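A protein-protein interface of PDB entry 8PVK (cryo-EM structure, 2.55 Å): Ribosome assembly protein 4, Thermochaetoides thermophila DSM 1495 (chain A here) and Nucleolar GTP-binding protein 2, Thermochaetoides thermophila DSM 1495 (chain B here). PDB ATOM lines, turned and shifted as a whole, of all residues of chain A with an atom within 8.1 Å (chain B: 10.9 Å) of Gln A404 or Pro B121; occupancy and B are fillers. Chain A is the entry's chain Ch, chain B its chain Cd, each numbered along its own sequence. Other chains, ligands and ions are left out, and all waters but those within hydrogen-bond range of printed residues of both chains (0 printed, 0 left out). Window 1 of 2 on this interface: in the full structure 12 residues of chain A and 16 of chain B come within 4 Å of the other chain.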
ATOM      1  N   ASP A 381      -9.065  13.912  -9.611  1.00  0.00           N
ATOM      2  CA  ASP A 381     -10.180  13.415  -8.821  1.00  0.00           C
ATOM      3  C   ASP A 381     -11.460  14.213  -9.050  1.00  0.00           C
ATOM      4  O   ASP A 381     -12.309  14.269  -8.154  1.00  0.00           O
ATOM      5  CB  ASP A 381      -9.814  13.371  -7.332  1.00  0.00           C
ATOM      6  CG  ASP A 381      -9.425  14.728  -6.760  1.00  0.00           C
ATOM      7  OD1 ASP A 381      -9.547  15.768  -7.439  1.00  0.00           O
ATOM      8  OD2 ASP A 381      -9.004  14.754  -5.588  1.00  0.00           O
ATOM      9  N   PHE A 382     -11.577  14.852 -10.216  1.00  0.00           N
ATOM     10  CA  PHE A 382     -12.725  15.608 -10.723  1.00  0.00           C
ATOM     11  C   PHE A 382     -12.921  16.925  -9.984  1.00  0.00           C
ATOM     12  O   PHE A 382     -13.968  17.564 -10.147  1.00  0.00           O
ATOM     13  CB  PHE A 382     -14.056  14.830 -10.676  1.00  0.00           C
ATOM     14  CG  PHE A 382     -14.101  13.547 -11.501  1.00  0.00           C
ATOM     15  CD1 PHE A 382     -13.011  13.075 -12.220  1.00  0.00           C
ATOM     16  CD2 PHE A 382     -15.278  12.819 -11.551  1.00  0.00           C
ATOM     17  CE1 PHE A 382     -13.092  11.910 -12.955  1.00  0.00           C
ATOM     18  CE2 PHE A 382     -15.366  11.655 -12.288  1.00  0.00           C
ATOM     19  CZ  PHE A 382     -14.272  11.201 -12.991  1.00  0.00           C
ATOM     20  N   THR A 383     -11.952  17.355  -9.175  1.00  0.00           N
ATOM     21  CA  THR A 383     -12.151  18.465  -8.254  1.00  0.00           C
ATOM     22  C   THR A 383     -11.049  19.507  -8.390  1.00  0.00           C
ATOM     23  O   THR A 383     -10.012  19.298  -9.041  1.00  0.00           O
ATOM     24  CB  THR A 383     -12.193  17.996  -6.790  1.00  0.00           C
ATOM     25  OG1 THR A 383     -10.929  17.427  -6.433  1.00  0.00           O
ATOM     26  CG2 THR A 383     -13.282  16.965  -6.569  1.00  0.00           C
ATOM     27  N   LEU A 401     -16.369  21.529  -6.568  1.00  0.00           N
ATOM     28  CA  LEU A 401     -17.017  20.322  -7.059  1.00  0.00           C
ATOM     29  C   LEU A 401     -17.999  20.683  -8.164  1.00  0.00           C
ATOM     30  O   LEU A 401     -18.607  21.757  -8.145  1.00  0.00           O
ATOM     31  CB  LEU A 401     -17.787  19.608  -5.939  1.00  0.00           C
ATOM     32  CG  LEU A 401     -17.115  19.273  -4.610  1.00  0.00           C
ATOM     33  CD1 LEU A 401     -18.173  19.022  -3.553  1.00  0.00           C
ATOM     34  CD2 LEU A 401     -16.250  18.051  -4.761  1.00  0.00           C
ATOM     35  N   GLY A 402     -18.193  19.761  -9.101  1.00  0.00           N
ATOM     36  CA  GLY A 402     -19.151  19.984 -10.166  1.00  0.00           C
ATOM     37  C   GLY A 402     -18.742  19.430 -11.514  1.00  0.00           C
ATOM     38  O   GLY A 402     -19.601  19.131 -12.347  1.00  0.00           O
ATOM     39  N   HIS A 403     -17.440  19.289 -11.744  1.00  0.00           N
ATOM     40  CA  HIS A 403     -16.970  18.636 -12.957  1.00  0.00           C
ATOM     41  C   HIS A 403     -17.259  17.142 -12.897  1.00  0.00           C
ATOM     42  O   HIS A 403     -17.115  16.506 -11.849  1.00  0.00           O
ATOM     43  CB  HIS A 403     -15.473  18.875 -13.149  1.00  0.00           C
ATOM     44  CG  HIS A 403     -15.146  20.171 -13.824  1.00  0.00           C
ATOM     45  ND1 HIS A 403     -15.216  20.337 -15.190  1.00  0.00           N
ATOM     46  CD2 HIS A 403     -14.735  21.359 -13.321  1.00  0.00           C
ATOM     47  CE1 HIS A 403     -14.868  21.573 -15.500  1.00  0.00           C
ATOM     48  NE2 HIS A 403     -14.570  22.214 -14.384  1.00  0.00           N
ATOM     49  N   GLN A 404     -17.675  16.581 -14.030  1.00  0.00           N
ATOM     50  CA  GLN A 404     -17.987  15.163 -14.133  1.00  0.00           C
ATOM     51  C   GLN A 404     -16.819  14.345 -14.662  1.00  0.00           C
ATOM     52  O   GLN A 404     -16.963  13.136 -14.868  1.00  0.00           O
ATOM     53  CB  GLN A 404     -19.213  14.955 -15.022  1.00  0.00           C
ATOM     54  CG  GLN A 404     -20.372  15.873 -14.695  1.00  0.00           C
ATOM     55  CD  GLN A 404     -21.066  15.488 -13.408  1.00  0.00           C
ATOM     56  OE1 GLN A 404     -20.857  16.111 -12.369  1.00  0.00           O
ATOM     57  NE2 GLN A 404     -21.895  14.454 -13.468  1.00  0.00           N
ATOM     58  N   ASN A 405     -15.671  14.974 -14.891  1.00  0.00           N
ATOM     59  CA  ASN A 405     -14.486  14.276 -15.364  1.00  0.00           C
ATOM     60  C   ASN A 405     -13.262  15.030 -14.865  1.00  0.00           C
ATOM     61  O   ASN A 405     -13.371  15.976 -14.079  1.00  0.00           O
ATOM     62  CB  ASN A 405     -14.495  14.140 -16.889  1.00  0.00           C
ATOM     63  CG  ASN A 405     -13.794  12.885 -17.366  1.00  0.00           C
ATOM     64  OD1 ASN A 405     -12.887  12.381 -16.706  1.00  0.00           O
ATOM     65  ND2 ASN A 405     -14.213  12.373 -18.514  1.00  0.00           N
ATOM     66  N   LYS A 406     -12.088  14.580 -15.306  1.00  0.00           N
ATOM     67  CA  LYS A 406     -10.830  15.164 -14.859  1.00  0.00           C
ATOM     68  C   LYS A 406     -10.718  16.609 -15.320  1.00  0.00           C
ATOM     69  O   LYS A 406     -11.193  16.973 -16.397  1.00  0.00           O
ATOM     70  CB  LYS A 406      -9.653  14.352 -15.397  1.00  0.00           C
ATOM     71  CG  LYS A 406      -9.796  12.853 -15.213  1.00  0.00           C
ATOM     72  CD  LYS A 406      -8.606  12.111 -15.795  1.00  0.00           C
ATOM     73  CE  LYS A 406      -8.613  12.154 -17.311  1.00  0.00           C
ATOM     74  NZ  LYS A 406      -9.734  11.358 -17.876  1.00  0.00           N
ATOM     75  N   VAL A 407     -10.100  17.443 -14.490  1.00  0.00           N
ATOM     76  CA  VAL A 407      -9.953  18.860 -14.784  1.00  0.00           C
ATOM     77  C   VAL A 407      -8.516  19.105 -15.212  1.00  0.00           C
ATOM     78  O   VAL A 407      -7.576  18.781 -14.476  1.00  0.00           O
ATOM     79  CB  VAL A 407     -10.325  19.727 -13.571  1.00  0.00           C
ATOM     80  CG1 VAL A 407     -10.104  21.192 -13.895  1.00  0.00           C
ATOM     81  CG2 VAL A 407     -11.751  19.462 -13.146  1.00  0.00           C
ATOM     82  N   GLY A 423     -12.430  21.128 -18.171  1.00  0.00           N
ATOM     83  CA  GLY A 423     -12.531  19.742 -17.780  1.00  0.00           C
ATOM     84  C   GLY A 423     -12.582  18.796 -18.969  1.00  0.00           C
ATOM     85  O   GLY A 423     -12.766  19.201 -20.122  1.00  0.00           O
ATOM     86  N   TRP A 424     -12.415  17.511 -18.661  1.00  0.00           N
ATOM     87  CA  TRP A 424     -12.558  16.445 -19.642  1.00  0.00           C
ATOM     88  C   TRP A 424     -14.009  16.039 -19.850  1.00  0.00           C
ATOM     89  O   TRP A 424     -14.277  15.140 -20.653  1.00  0.00           O
ATOM     90  CB  TRP A 424     -11.728  15.228 -19.225  1.00  0.00           C
ATOM     91  CG  TRP A 424     -10.247  15.406 -19.405  1.00  0.00           C
ATOM     92  CD1 TRP A 424      -9.472  16.411 -18.904  1.00  0.00           C
ATOM     93  CD2 TRP A 424      -9.363  14.543 -20.127  1.00  0.00           C
ATOM     94  NE1 TRP A 424      -8.164  16.231 -19.275  1.00  0.00           N
ATOM     95  CE2 TRP A 424      -8.069  15.091 -20.027  1.00  0.00           C
ATOM     96  CE3 TRP A 424      -9.539  13.361 -20.853  1.00  0.00           C
ATOM     97  CZ2 TRP A 424      -6.960  14.499 -20.622  1.00  0.00           C
ATOM     98  CZ3 TRP A 424      -8.437  12.775 -21.443  1.00  0.00           C
ATOM     99  CH2 TRP A 424      -7.164  13.344 -21.324  1.00  0.00           C
ATOM    100  N   ASP A 425     -14.944  16.677 -19.141  1.00  0.00           N
ATOM    101  CA  ASP A 425     -16.374  16.494 -19.351  1.00  0.00           C
ATOM    102  C   ASP A 425     -16.940  17.492 -20.351  1.00  0.00           C
ATOM    103  O   ASP A 425     -18.098  17.912 -20.213  1.00  0.00           O
ATOM    104  CB  ASP A 425     -17.119  16.595 -18.020  1.00  0.00           C
ATOM    105  CG  ASP A 425     -16.727  17.821 -17.225  1.00  0.00           C
ATOM    106  OD1 ASP A 425     -15.706  18.452 -17.565  1.00  0.00           O
ATOM    107  OD2 ASP A 425     -17.443  18.159 -16.261  1.00  0.00           O
ATOM    108  N   ASN A 426     -16.119  17.919 -21.315  1.00  0.00           N
ATOM    109  CA  ASN A 426     -16.486  18.765 -22.450  1.00  0.00           C
ATOM    110  C   ASN A 426     -16.902  20.169 -22.025  1.00  0.00           C
ATOM    111  O   ASN A 426     -17.589  20.864 -22.779  1.00  0.00           O
ATOM    112  CB  ASN A 426     -17.608  18.133 -23.290  1.00  0.00           C
ATOM    113  CG  ASN A 426     -17.266  16.742 -23.778  1.00  0.00           C
ATOM    114  OD1 ASN A 426     -16.121  16.445 -24.092  1.00  0.00           O
ATOM    115  ND2 ASN A 426     -18.272  15.881 -23.850  1.00  0.00           N
ATOM    116  N   SER A 427     -16.503  20.623 -20.837  1.00  0.00           N
ATOM    117  CA  SER A 427     -17.077  21.843 -20.288  1.00  0.00           C
ATOM    118  C   SER A 427     -16.032  22.702 -19.590  1.00  0.00           C
ATOM    119  O   SER A 427     -15.034  22.209 -19.052  1.00  0.00           O
ATOM    120  CB  SER A 427     -18.211  21.525 -19.304  1.00  0.00           C
ATOM    121  OG  SER A 427     -17.699  21.071 -18.065  1.00  0.00           O
ATOM    122  N   LYS A 429     -16.006  25.693 -16.559  1.00  0.00           N
ATOM    123  CA  LYS A 429     -16.819  26.145 -15.442  1.00  0.00           C
ATOM    124  C   LYS A 429     -16.215  27.389 -14.804  1.00  0.00           C
ATOM    125  O   LYS A 429     -14.992  27.574 -14.787  1.00  0.00           O
ATOM    126  CB  LYS A 429     -16.977  25.042 -14.392  1.00  0.00           C
ATOM    127  CG  LYS A 429     -17.902  23.921 -14.823  1.00  0.00           C
ATOM    128  CD  LYS A 429     -18.110  22.913 -13.712  1.00  0.00           C
ATOM    129  CE  LYS A 429     -19.321  22.042 -13.989  1.00  0.00           C
ATOM    130  NZ  LYS A 429     -19.163  21.257 -15.241  1.00  0.00           N
ATOM    131  N   ASN A 441     -21.978  27.312 -16.044  1.00  0.00           N
ATOM    132  CA  ASN A 441     -21.321  26.330 -16.894  1.00  0.00           C
ATOM    133  C   ASN A 441     -21.287  26.842 -18.327  1.00  0.00           C
ATOM    134  O   ASN A 441     -22.307  27.299 -18.851  1.00  0.00           O
ATOM    135  CB  ASN A 441     -22.050  24.987 -16.832  1.00  0.00           C
ATOM    136  CG  ASN A 441     -21.345  23.903 -17.620  1.00  0.00           C
ATOM    137  OD1 ASN A 441     -20.129  23.945 -17.806  1.00  0.00           O
ATOM    138  ND2 ASN A 441     -22.107  22.926 -18.094  1.00  0.00           N
ATOM    139  N   MET B 114     -29.873  14.019 -28.655  1.00  0.00           N
ATOM    140  CA  MET B 114     -30.215  14.075 -27.234  1.00  0.00           C
ATOM    141  C   MET B 114     -28.995  14.092 -26.327  1.00  0.00           C
ATOM    142  O   MET B 114     -29.036  14.716 -25.263  1.00  0.00           O
ATOM    143  CB  MET B 114     -31.116  12.896 -26.865  1.00  0.00           C
ATOM    144  CG  MET B 114     -32.501  12.886 -27.495  1.00  0.00           C
ATOM    145  SD  MET B 114     -33.494  14.313 -26.991  1.00  0.00           S
ATOM    146  CE  MET B 114     -33.399  15.384 -28.411  1.00  0.00           C
ATOM    147  N   SER B 115     -27.905  13.427 -26.718  1.00  0.00           N
ATOM    148  CA  SER B 115     -26.705  13.432 -25.888  1.00  0.00           C
ATOM    149  C   SER B 115     -26.098  14.826 -25.780  1.00  0.00           C
ATOM    150  O   SER B 115     -25.481  15.153 -24.760  1.00  0.00           O
ATOM    151  CB  SER B 115     -25.678  12.446 -26.439  1.00  0.00           C
ATOM    152  OG  SER B 115     -25.168  12.888 -27.682  1.00  0.00           O
ATOM    153  N   ILE B 117     -28.125  17.624 -26.262  1.00  0.00           N
ATOM    154  CA  ILE B 117     -29.216  18.518 -25.887  1.00  0.00           C
ATOM    155  C   ILE B 117     -29.574  18.389 -24.409  1.00  0.00           C
ATOM    156  O   ILE B 117     -29.667  19.392 -23.700  1.00  0.00           O
ATOM    157  CB  ILE B 117     -30.454  18.294 -26.786  1.00  0.00           C
ATOM    158  CG1 ILE B 117     -30.154  18.741 -28.217  1.00  0.00           C
ATOM    159  CG2 ILE B 117     -31.661  19.046 -26.249  1.00  0.00           C
ATOM    160  CD1 ILE B 117     -31.239  18.398 -29.202  1.00  0.00           C
ATOM    161  N   ARG B 118     -29.777  17.165 -23.923  1.00  0.00           N
ATOM    162  CA  ARG B 118     -30.227  16.992 -22.547  1.00  0.00           C
ATOM    163  C   ARG B 118     -29.102  17.300 -21.564  1.00  0.00           C
ATOM    164  O   ARG B 118     -27.915  17.238 -21.898  1.00  0.00           O
ATOM    165  CB  ARG B 118     -30.752  15.575 -22.305  1.00  0.00           C
ATOM    166  CG  ARG B 118     -29.680  14.510 -22.142  1.00  0.00           C
ATOM    167  CD  ARG B 118     -30.283  13.135 -21.898  1.00  0.00           C
ATOM    168  NE  ARG B 118     -31.030  12.630 -23.044  1.00  0.00           N
ATOM    169  CZ  ARG B 118     -32.352  12.537 -23.091  1.00  0.00           C
ATOM    170  NH1 ARG B 118     -33.109  12.921 -22.076  1.00  0.00           N
ATOM    171  NH2 ARG B 118     -32.930  12.042 -24.181  1.00  0.00           N
ATOM    172  N   ASP B 119     -29.492  17.654 -20.343  1.00  0.00           N
ATOM    173  CA  ASP B 119     -28.529  18.041 -19.326  1.00  0.00           C
ATOM    174  C   ASP B 119     -27.782  16.828 -18.772  1.00  0.00           C
ATOM    175  O   ASP B 119     -28.218  15.679 -18.893  1.00  0.00           O
ATOM    176  CB  ASP B 119     -29.222  18.834 -18.209  1.00  0.00           C
ATOM    177  CG  ASP B 119     -30.295  18.035 -17.461  1.00  0.00           C
ATOM    178  OD1 ASP B 119     -30.576  16.865 -17.798  1.00  0.00           O
ATOM    179  OD2 ASP B 119     -30.873  18.600 -16.509  1.00  0.00           O
ATOM    180  N   GLY B 120     -26.630  17.100 -18.167  1.00  0.00           N
ATOM    181  CA  GLY B 120     -25.813  16.067 -17.579  1.00  0.00           C
ATOM    182  C   GLY B 120     -26.363  15.585 -16.253  1.00  0.00           C
ATOM    183  O   GLY B 120     -27.333  16.132 -15.718  1.00  0.00           O
ATOM    184  N   PRO B 121     -25.747  14.547 -15.692  1.00  0.00           N
ATOM    185  CA  PRO B 121     -26.224  14.006 -14.415  1.00  0.00           C
ATOM    186  C   PRO B 121     -25.755  14.858 -13.245  1.00  0.00           C
ATOM    187  O   PRO B 121     -25.019  15.836 -13.395  1.00  0.00           O
ATOM    188  CB  PRO B 121     -25.618  12.601 -14.364  1.00  0.00           C
ATOM    189  CG  PRO B 121     -24.520  12.582 -15.398  1.00  0.00           C
ATOM    190  CD  PRO B 121     -24.531  13.870 -16.168  1.00  0.00           C
ATOM    191  N   LYS B 122     -26.211  14.472 -12.057  1.00  0.00           N
ATOM    192  CA  LYS B 122     -25.837  15.180 -10.842  1.00  0.00           C
ATOM    193  C   LYS B 122     -24.373  14.923 -10.499  1.00  0.00           C
ATOM    194  O   LYS B 122     -23.790  13.905 -10.884  1.00  0.00           O
ATOM    195  CB  LYS B 122     -26.736  14.756  -9.681  1.00  0.00           C
ATOM    196  CG  LYS B 122     -28.222  14.884  -9.976  1.00  0.00           C
ATOM    197  CD  LYS B 122     -29.065  14.341  -8.834  1.00  0.00           C
ATOM    198  CE  LYS B 122     -30.548  14.444  -9.151  1.00  0.00           C
ATOM    199  NZ  LYS B 122     -31.393  13.883  -8.061  1.00  0.00           N
ATOM    200  N   LEU B 123     -23.777  15.874  -9.774  1.00  0.00           N
ATOM    201  CA  LEU B 123     -22.355  15.783  -9.451  1.00  0.00           C
ATOM    202  C   LEU B 123     -22.059  14.644  -8.481  1.00  0.00           C
ATOM    203  O   LEU B 123     -21.013  13.993  -8.594  1.00  0.00           O
ATOM    204  CB  LEU B 123     -21.860  17.134  -8.918  1.00  0.00           C
ATOM    205  CG  LEU B 123     -22.404  17.804  -7.646  1.00  0.00           C
ATOM    206  CD1 LEU B 123     -21.762  17.302  -6.354  1.00  0.00           C
ATOM    207  CD2 LEU B 123     -22.269  19.316  -7.758  1.00  0.00           C
ATOM    208  N   GLU B 124     -22.966  14.380  -7.536  1.00  0.00           N
ATOM    209  CA  GLU B 124     -22.770  13.255  -6.628  1.00  0.00           C
ATOM    210  C   GLU B 124     -22.847  11.924  -7.370  1.00  0.00           C
ATOM    211  O   GLU B 124     -22.072  11.006  -7.079  1.00  0.00           O
ATOM    212  CB  GLU B 124     -23.772  13.333  -5.468  1.00  0.00           C
ATOM    213  CG  GLU B 124     -25.256  13.301  -5.831  1.00  0.00           C
ATOM    214  CD  GLU B 124     -25.819  11.899  -5.947  1.00  0.00           C
ATOM    215  OE1 GLU B 124     -25.199  10.959  -5.407  1.00  0.00           O
ATOM    216  OE2 GLU B 124     -26.888  11.740  -6.573  1.00  0.00           O
ATOM    217  N   ASP B 125     -23.739  11.814  -8.360  1.00  0.00           N
ATOM    218  CA  ASP B 125     -23.787  10.609  -9.182  1.00  0.00           C
ATOM    219  C   ASP B 125     -22.539  10.474 -10.047  1.00  0.00           C
ATOM    220  O   ASP B 125     -22.020   9.367 -10.225  1.00  0.00           O
ATOM    221  CB  ASP B 125     -25.042  10.610 -10.054  1.00  0.00           C
ATOM    222  CG  ASP B 125     -26.294  10.260  -9.277  1.00  0.00           C
ATOM    223  OD1 ASP B 125     -26.191   9.487  -8.302  1.00  0.00           O
ATOM    224  OD2 ASP B 125     -27.381  10.754  -9.644  1.00  0.00           O
ATOM    225  N   GLY B 126     -22.049  11.591 -10.589  1.00  0.00           N
ATOM    226  CA  GLY B 126     -20.843  11.545 -11.401  1.00  0.00           C
ATOM    227  C   GLY B 126     -19.614  11.143 -10.606  1.00  0.00           C
ATOM    228  O   GLY B 126     -18.725  10.461 -11.124  1.00  0.00           O
ATOM    229  N   LEU B 127     -19.544  11.561  -9.340  1.00  0.00           N
ATOM    230  CA  LEU B 127     -18.447  11.118  -8.485  1.00  0.00           C
ATOM    231  C   LEU B 127     -18.631   9.667  -8.046  1.00  0.00           C
ATOM    232  O   LEU B 127     -17.652   8.919  -7.933  1.00  0.00           O
ATOM    233  CB  LEU B 127     -18.327  12.036  -7.269  1.00  0.00           C
ATOM    234  CG  LEU B 127     -17.869  13.468  -7.550  1.00  0.00           C
ATOM    235  CD1 LEU B 127     -17.957  14.315  -6.292  1.00  0.00           C
ATOM    236  CD2 LEU B 127     -16.457  13.480  -8.107  1.00  0.00           C
ATOM    237  N   LYS B 128     -19.878   9.259  -7.787  1.00  0.00           N
ATOM    238  CA  LYS B 128     -20.148   7.907  -7.314  1.00  0.00           C
ATOM    239  C   LYS B 128     -19.892   6.865  -8.395  1.00  0.00           C
ATOM    240  O   LYS B 128     -19.478   5.742  -8.085  1.00  0.00           O
ATOM    241  CB  LYS B 128     -21.590   7.817  -6.812  1.00  0.00           C
ATOM    242  CG  LYS B 128     -21.932   6.537  -6.072  1.00  0.00           C
ATOM    243  CD  LYS B 128     -23.377   6.551  -5.602  1.00  0.00           C
ATOM    244  CE  LYS B 128     -23.703   5.318  -4.777  1.00  0.00           C
ATOM    245  NZ  LYS B 128     -23.642   4.074  -5.594  1.00  0.00           N
ATOM    246  N   LYS B 129     -20.119   7.216  -9.665  1.00  0.00           N
ATOM    247  CA  LYS B 129     -19.845   6.281 -10.751  1.00  0.00           C
ATOM    248  C   LYS B 129     -18.355   6.048 -10.974  1.00  0.00           C
ATOM    249  O   LYS B 129     -17.994   5.113 -11.694  1.00  0.00           O
ATOM    250  CB  LYS B 129     -20.480   6.772 -12.054  1.00  0.00           C
ATOM    251  CG  LYS B 129     -21.997   6.718 -12.077  1.00  0.00           C
ATOM    252  CD  LYS B 129     -22.543   7.355 -13.343  1.00  0.00           C
ATOM    253  CE  LYS B 129     -22.252   6.502 -14.566  1.00  0.00           C
ATOM    254  NZ  LYS B 129     -22.882   7.065 -15.791  1.00  0.00           N
ATOM    255  N   HIS B 130     -17.485   6.868 -10.384  1.00  0.00           N
ATOM    256  CA  HIS B 130     -16.052   6.739 -10.593  1.00  0.00           C
ATOM    257  C   HIS B 130     -15.248   6.564  -9.311  1.00  0.00           C
ATOM    258  O   HIS B 130     -14.021   6.450  -9.394  1.00  0.00           O
ATOM    259  CB  HIS B 130     -15.517   7.956 -11.358  1.00  0.00           C
ATOM    260  CG  HIS B 130     -16.087   8.102 -12.733  1.00  0.00           C
ATOM    261  ND1 HIS B 130     -17.231   8.825 -12.993  1.00  0.00           N
ATOM    262  CD2 HIS B 130     -15.672   7.614 -13.926  1.00  0.00           C
ATOM    263  CE1 HIS B 130     -17.495   8.778 -14.286  1.00  0.00           C
ATOM    264  NE2 HIS B 130     -16.564   8.050 -14.876  1.00  0.00           N
ATOM    265  N   GLN B 131     -15.898   6.550  -8.139  1.00  0.00           N
ATOM    266  CA  GLN B 131     -15.170   6.386  -6.879  1.00  0.00           C
ATOM    267  C   GLN B 131     -14.409   5.064  -6.810  1.00  0.00           C
ATOM    268  O   GLN B 131     -13.259   5.032  -6.357  1.00  0.00           O
ATOM    269  CB  GLN B 131     -16.129   6.493  -5.693  1.00  0.00           C
ATOM    270  CG  GLN B 131     -16.333   7.901  -5.172  1.00  0.00           C
ATOM    271  CD  GLN B 131     -15.026   8.600  -4.864  1.00  0.00           C
ATOM    272  OE1 GLN B 131     -14.631   9.533  -5.562  1.00  0.00           O
ATOM    273  NE2 GLN B 131     -14.348   8.151  -3.816  1.00  0.00           N
ATOM    274  N   LYS B 133     -13.311   2.999  -9.317  1.00  0.00           N
ATOM    275  CA  LYS B 133     -12.186   3.024 -10.244  1.00  0.00           C
ATOM    276  C   LYS B 133     -11.097   3.976  -9.772  1.00  0.00           C
ATOM    277  O   LYS B 133      -9.907   3.694  -9.950  1.00  0.00           O
ATOM    278  CB  LYS B 133     -12.669   3.416 -11.640  1.00  0.00           C
ATOM    279  CG  LYS B 133     -11.630   3.247 -12.733  1.00  0.00           C
ATOM    280  CD  LYS B 133     -12.209   3.577 -14.097  1.00  0.00           C
ATOM    281  CE  LYS B 133     -11.190   3.345 -15.198  1.00  0.00           C
ATOM    282  NZ  LYS B 133     -10.068   4.320 -15.126  1.00  0.00           N
ATOM    283  N   MET B 134     -11.483   5.089  -9.145  1.00  0.00           N
ATOM    284  CA  MET B 134     -10.512   6.048  -8.635  1.00  0.00           C
ATOM    285  C   MET B 134      -9.707   5.462  -7.480  1.00  0.00           C
ATOM    286  O   MET B 134      -8.487   5.651  -7.410  1.00  0.00           O
ATOM    287  CB  MET B 134     -11.249   7.312  -8.204  1.00  0.00           C
ATOM    288  CG  MET B 134     -10.389   8.467  -7.765  1.00  0.00           C
ATOM    289  SD  MET B 134     -11.479   9.826  -7.324  1.00  0.00           S
ATOM    290  CE  MET B 134     -12.054  10.299  -8.954  1.00  0.00           C
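The backbone carbonyl oxygen of Gly B126 lies within hydrogen-bond range of a ring nitrogen (ND1) of His B130 (2.9 Å).
The side-chain carboxylate (OD2) of Asp A425 lies within hydrogen-bond range of the backbone NH (N) of Gln A404 (2.7 Å).
O of Gly A402 sits close to OE1 of Gln A404, 3.3 Å away.
The side-chain carboxylate (OD1) of Asp A381 lies close to the backbone NH (N) of Thr A383.
The side-chain amide oxygen (OE1) of Gln B131 lies close to the side-chain sulfur (SD) of Met B134, 3.6 Å away.
Asp A381 touches Met B134.
Gly B126 touches Phe A382 (O to CE2, 3.8 Å).
Phe A382 touches Leu B127.
ND1 of His B130 touches CE2 of Phe A382 (3.5 Å).
CD2 of Leu B123 touches CA of Gly A402, at 3.996 Å.
CA of Leu B123 touches OE1 of Gln A404, 3.3 Å away.
Gln A404 touches Gly B126 (NE2 to CA, 3.7 Å).
The backbone carbonyl oxygen (O) of Lys B122 is in hydrogen-bond range of the side-chain amide nitrogen (NE2) of Gln A404 (3.3 Å).
The backbone carbonyl oxygen (O) of Pro B121 sits at hydrogen-bond distance from the side-chain amide nitrogen (NE2) of Gln A404 (3.4 Å).
Of chain B, only Pro B121 (3.4 Å), Lys B122 (3.3 Å), Leu B123 (3.3 Å) and Gly B126 (3.7 Å) come within 4 Å of Gln A404.
Pro B121 touches just one residue of chain A: Gln A404.
No residue of chain B comes within 4 Å of His A403.
No residue of chain B comes within 4 Å of Asn A405.
No residue of chain B comes within 4 Å of Asp A425.
Printed residues of chain A within 4 Å of Gly B126: Phe A382 (3.8 Å) and Gln A404 (3.7 Å).
Of the printed residues of chain A, Met B134 touches Asp A381.
Of the printed residues of chain A, Leu B123 touches Gly A402 and Gln A404.
Printed residues of chain B within 4 Å of Phe A382: Gly B126, Leu B127 and His B130.
Of the printed residues of chain B, Gly A402 touches Leu B123 (3.996 Å).
Leu A401 touches none of the printed residues of chain B.
The nearest residue of chain B that does not touch Gln A404 is His B130 (4.4 Å).
Printed residues of chain A that touch a printed residue of chain B: Asp A381, Phe A382, Gly A402 and Gln A404.
Among the printed residues, no Asp or Glu carboxylate lies within 4 Å of a Lys or Arg side-chain nitrogen of the other chain.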
